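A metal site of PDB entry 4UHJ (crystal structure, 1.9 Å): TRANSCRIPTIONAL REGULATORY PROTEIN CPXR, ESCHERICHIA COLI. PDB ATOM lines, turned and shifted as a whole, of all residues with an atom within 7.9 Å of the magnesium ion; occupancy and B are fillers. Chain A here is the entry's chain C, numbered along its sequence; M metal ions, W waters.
Asp 8 touches the magnesium ion (OD1 to MG, 3.9 Å).
The nearest printed residue that does not touch the magnesium ion is Met 54 (4.4 Å).
Water W1 lies within hydrogen-bond range of the side-chain carboxylate (OD1) of Asp 8 (2.7 Å), the side-chain carboxylate (OD1) of Asp 51 (3.5 Å) and the side-chain amino group (NZ) of Lys 100 (3.5 Å).
Water W1 is bound to the magnesium ion (2.0 Å).
The magnesium ion is bound by OD2 of Asp 51 (2.1 Å).
The magnesium ion is bound by the backbone carbonyl oxygen (O) of Met 53.
The magnesium ion is bound by OD1 of Asp 9, 2.3 Å away.
The magnesium ion has four donor atoms within binding distance.
OD1 of Asp 8 lies within hydrogen-bond range of N of Asp 10, at 2.8 Å.
The backbone carbonyl oxygen (O) of Val 7 is in hydrogen-bond range of the backbone NH (N) of Asp 51.
The side-chain amino group (NZ) of Lys 100 is in salt-bridge range of the side-chain carboxylate (OD2) of Asp 8 (2.8 Å).
The side-chain carboxylate (OD1) of Asp 51 is in salt-bridge range of the side-chain amino group (NZ) of Lys 100, 3.8 Å away.
A ring nitrogen (ND1) of His 32 sits at hydrogen-bond distance from the backbone carbonyl oxygen (O) of Asp 8, at 3.0 Å.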
ATOM      1  N   VAL A   7     -22.805 -16.115  -4.484  1.00  0.00           N
ATOM      2  CA  VAL A   7     -23.007 -14.676  -4.730  1.00  0.00           C
ATOM      3  C   VAL A   7     -22.865 -14.379  -6.218  1.00  0.00           C
ATOM      4  O   VAL A   7     -21.768 -14.402  -6.762  1.00  0.00           O
ATOM      5  CB  VAL A   7     -22.029 -13.793  -3.899  1.00  0.00           C
ATOM      6  CG1 VAL A   7     -22.416 -12.316  -3.988  1.00  0.00           C
ATOM      7  CG2 VAL A   7     -21.925 -14.277  -2.447  1.00  0.00           C
ATOM      8  N   ASP A   8     -23.994 -14.068  -6.869  1.00  0.00           N
ATOM      9  CA  ASP A   8     -24.054 -13.744  -8.287  1.00  0.00           C
ATOM     10  C   ASP A   8     -25.369 -13.055  -8.565  1.00  0.00           C
ATOM     11  O   ASP A   8     -26.381 -13.440  -7.996  1.00  0.00           O
ATOM     12  CB  ASP A   8     -23.902 -15.031  -9.133  1.00  0.00           C
ATOM     13  CG  ASP A   8     -23.531 -14.825 -10.589  1.00  0.00           C
ATOM     14  OD1 ASP A   8     -24.221 -14.031 -11.276  1.00  0.00           O
ATOM     15  OD2 ASP A   8     -22.584 -15.481 -11.056  1.00  0.00           O
ATOM     16  N   ASP A   9     -25.345 -12.013  -9.433  1.00  0.00           N
ATOM     17  CA  ASP A   9     -26.550 -11.252  -9.788  1.00  0.00           C
ATOM     18  C   ASP A   9     -27.411 -12.006 -10.826  1.00  0.00           C
ATOM     19  O   ASP A   9     -28.580 -11.669 -10.980  1.00  0.00           O
ATOM     20  CB  ASP A   9     -26.182  -9.859 -10.304  1.00  0.00           C
ATOM     21  CG  ASP A   9     -25.288  -9.852 -11.524  1.00  0.00           C
ATOM     22  OD1 ASP A   9     -24.216 -10.478 -11.475  1.00  0.00           O
ATOM     23  OD2 ASP A   9     -25.664  -9.230 -12.534  1.00  0.00           O
ATOM     24  N   ASP A  10     -26.841 -13.016 -11.515  1.00  0.00           N
ATOM     25  CA  ASP A  10     -27.575 -13.822 -12.506  1.00  0.00           C
ATOM     26  C   ASP A  10     -28.445 -14.841 -11.755  1.00  0.00           C
ATOM     27  O   ASP A  10     -27.945 -15.886 -11.319  1.00  0.00           O
ATOM     28  CB  ASP A  10     -26.601 -14.513 -13.497  1.00  0.00           C
ATOM     29  CG  ASP A  10     -27.245 -15.315 -14.625  1.00  0.00           C
ATOM     30  OD1 ASP A  10     -28.481 -15.513 -14.587  1.00  0.00           O
ATOM     31  OD2 ASP A  10     -26.518 -15.750 -15.529  1.00  0.00           O
ATOM     32  N   LEU A  13     -28.472 -18.406 -13.244  1.00  0.00           N
ATOM     33  CA  LEU A  13     -27.300 -19.185 -12.861  1.00  0.00           C
ATOM     34  C   LEU A  13     -27.380 -19.648 -11.398  1.00  0.00           C
ATOM     35  O   LEU A  13     -27.105 -20.820 -11.132  1.00  0.00           O
ATOM     36  CB  LEU A  13     -25.995 -18.418 -13.117  1.00  0.00           C
ATOM     37  CG  LEU A  13     -24.687 -19.125 -12.689  1.00  0.00           C
ATOM     38  CD1 LEU A  13     -24.482 -20.463 -13.426  1.00  0.00           C
ATOM     39  CD2 LEU A  13     -23.508 -18.243 -12.891  1.00  0.00           C
ATOM     40  N   HIS A  32     -27.511 -11.815  -4.181  1.00  0.00           N
ATOM     41  CA  HIS A  32     -27.513 -11.343  -5.567  1.00  0.00           C
ATOM     42  C   HIS A  32     -26.633 -10.101  -5.803  1.00  0.00           C
ATOM     43  O   HIS A  32     -26.576  -9.609  -6.929  1.00  0.00           O
ATOM     44  CB  HIS A  32     -28.950 -11.122  -6.048  1.00  0.00           C
ATOM     45  CG  HIS A  32     -29.678 -12.432  -6.140  1.00  0.00           C
ATOM     46  ND1 HIS A  32     -29.203 -13.462  -6.951  1.00  0.00           N
ATOM     47  CD2 HIS A  32     -30.804 -12.844  -5.517  1.00  0.00           C
ATOM     48  CE1 HIS A  32     -30.059 -14.468  -6.800  1.00  0.00           C
ATOM     49  NE2 HIS A  32     -31.036 -14.147  -5.952  1.00  0.00           N
ATOM     50  N   ASP A  51     -19.129 -13.977  -7.710  1.00  0.00           N
ATOM     51  CA  ASP A  51     -19.175 -13.392  -9.048  1.00  0.00           C
ATOM     52  C   ASP A  51     -18.323 -12.102  -9.091  1.00  0.00           C
ATOM     53  O   ASP A  51     -18.353 -11.312  -8.149  1.00  0.00           O
ATOM     54  CB  ASP A  51     -20.634 -13.088  -9.422  1.00  0.00           C
ATOM     55  CG  ASP A  51     -20.900 -12.462 -10.777  1.00  0.00           C
ATOM     56  OD1 ASP A  51     -20.038 -12.585 -11.677  1.00  0.00           O
ATOM     57  OD2 ASP A  51     -22.002 -11.951 -10.979  1.00  0.00           O
ATOM     58  N   VAL A  52     -17.556 -11.904 -10.173  1.00  0.00           N
ATOM     59  CA  VAL A  52     -16.658 -10.754 -10.309  1.00  0.00           C
ATOM     60  C   VAL A  52     -17.433  -9.451 -10.600  1.00  0.00           C
ATOM     61  O   VAL A  52     -17.196  -8.447  -9.941  1.00  0.00           O
ATOM     62  CB  VAL A  52     -15.524 -11.011 -11.352  1.00  0.00           C
ATOM     63  CG1 VAL A  52     -14.751  -9.749 -11.697  1.00  0.00           C
ATOM     64  CG2 VAL A  52     -14.562 -12.098 -10.867  1.00  0.00           C
ATOM     65  N   MET A  53     -18.379  -9.482 -11.545  1.00  0.00           N
ATOM     66  CA  MET A  53     -19.157  -8.319 -12.001  1.00  0.00           C
ATOM     67  C   MET A  53     -20.593  -8.359 -11.483  1.00  0.00           C
ATOM     68  O   MET A  53     -21.379  -9.211 -11.888  1.00  0.00           O
ATOM     69  CB  MET A  53     -19.127  -8.260 -13.541  1.00  0.00           C
ATOM     70  CG  MET A  53     -19.656  -6.964 -14.107  1.00  0.00           C
ATOM     71  SD  MET A  53     -19.444  -6.786 -15.903  1.00  0.00           S
ATOM     72  CE  MET A  53     -17.648  -6.988 -16.052  1.00  0.00           C
ATOM     73  N   MET A  54     -20.950  -7.415 -10.577  1.00  0.00           N
ATOM     74  CA  MET A  54     -22.277  -7.304  -9.968  1.00  0.00           C
ATOM     75  C   MET A  54     -22.654  -5.854  -9.691  1.00  0.00           C
ATOM     76  O   MET A  54     -21.751  -5.063  -9.406  1.00  0.00           O
ATOM     77  CB  MET A  54     -22.328  -8.054  -8.611  1.00  0.00           C
ATOM     78  CG  MET A  54     -22.069  -9.523  -8.660  1.00  0.00           C
ATOM     79  SD  MET A  54     -22.238 -10.212  -7.004  1.00  0.00           S
ATOM     80  CE  MET A  54     -20.722  -9.616  -6.226  1.00  0.00           C
ATOM     81  N   PRO A  55     -23.961  -5.499  -9.606  1.00  0.00           N
ATOM     82  CA  PRO A  55     -24.313  -4.129  -9.195  1.00  0.00           C
ATOM     83  C   PRO A  55     -24.158  -3.952  -7.664  1.00  0.00           C
ATOM     84  O   PRO A  55     -23.990  -4.955  -6.950  1.00  0.00           O
ATOM     85  CB  PRO A  55     -25.765  -3.967  -9.644  1.00  0.00           C
ATOM     86  CG  PRO A  55     -26.318  -5.360  -9.686  1.00  0.00           C
ATOM     87  CD  PRO A  55     -25.165  -6.325  -9.851  1.00  0.00           C
ATOM     88  N   LEU A  77     -15.927 -16.408  -9.516  1.00  0.00           N
ATOM     89  CA  LEU A  77     -16.663 -16.835 -10.719  1.00  0.00           C
ATOM     90  C   LEU A  77     -16.510 -15.746 -11.775  1.00  0.00           C
ATOM     91  O   LEU A  77     -16.924 -14.602 -11.542  1.00  0.00           O
ATOM     92  CB  LEU A  77     -18.162 -17.072 -10.429  1.00  0.00           C
ATOM     93  CG  LEU A  77     -18.535 -17.952  -9.215  1.00  0.00           C
ATOM     94  CD1 LEU A  77     -20.056 -17.979  -9.008  1.00  0.00           C
ATOM     95  CD2 LEU A  77     -17.926 -19.364  -9.314  1.00  0.00           C
ATOM     96  N   LYS A 100     -16.432 -19.063 -16.274  1.00  0.00           N
ATOM     97  CA  LYS A 100     -17.702 -19.425 -16.898  1.00  0.00           C
ATOM     98  C   LYS A 100     -17.582 -19.344 -18.428  1.00  0.00           C
ATOM     99  O   LYS A 100     -16.833 -18.535 -18.984  1.00  0.00           O
ATOM    100  CB  LYS A 100     -18.866 -18.524 -16.395  1.00  0.00           C
ATOM    101  CG  LYS A 100     -19.291 -18.736 -14.939  1.00  0.00           C
ATOM    102  CD  LYS A 100     -20.450 -17.837 -14.542  1.00  0.00           C
ATOM    103  CE  LYS A 100     -20.028 -16.497 -13.985  1.00  0.00           C
ATOM    104  NZ  LYS A 100     -21.192 -15.694 -13.522  1.00  0.00           N
HETATM  105 MG    MG M   1     -22.385 -10.938 -12.811  1.00  0.00          MG
HETATM  106  O   HOH W   1     -23.055 -12.765 -13.358  1.00  0.00           O
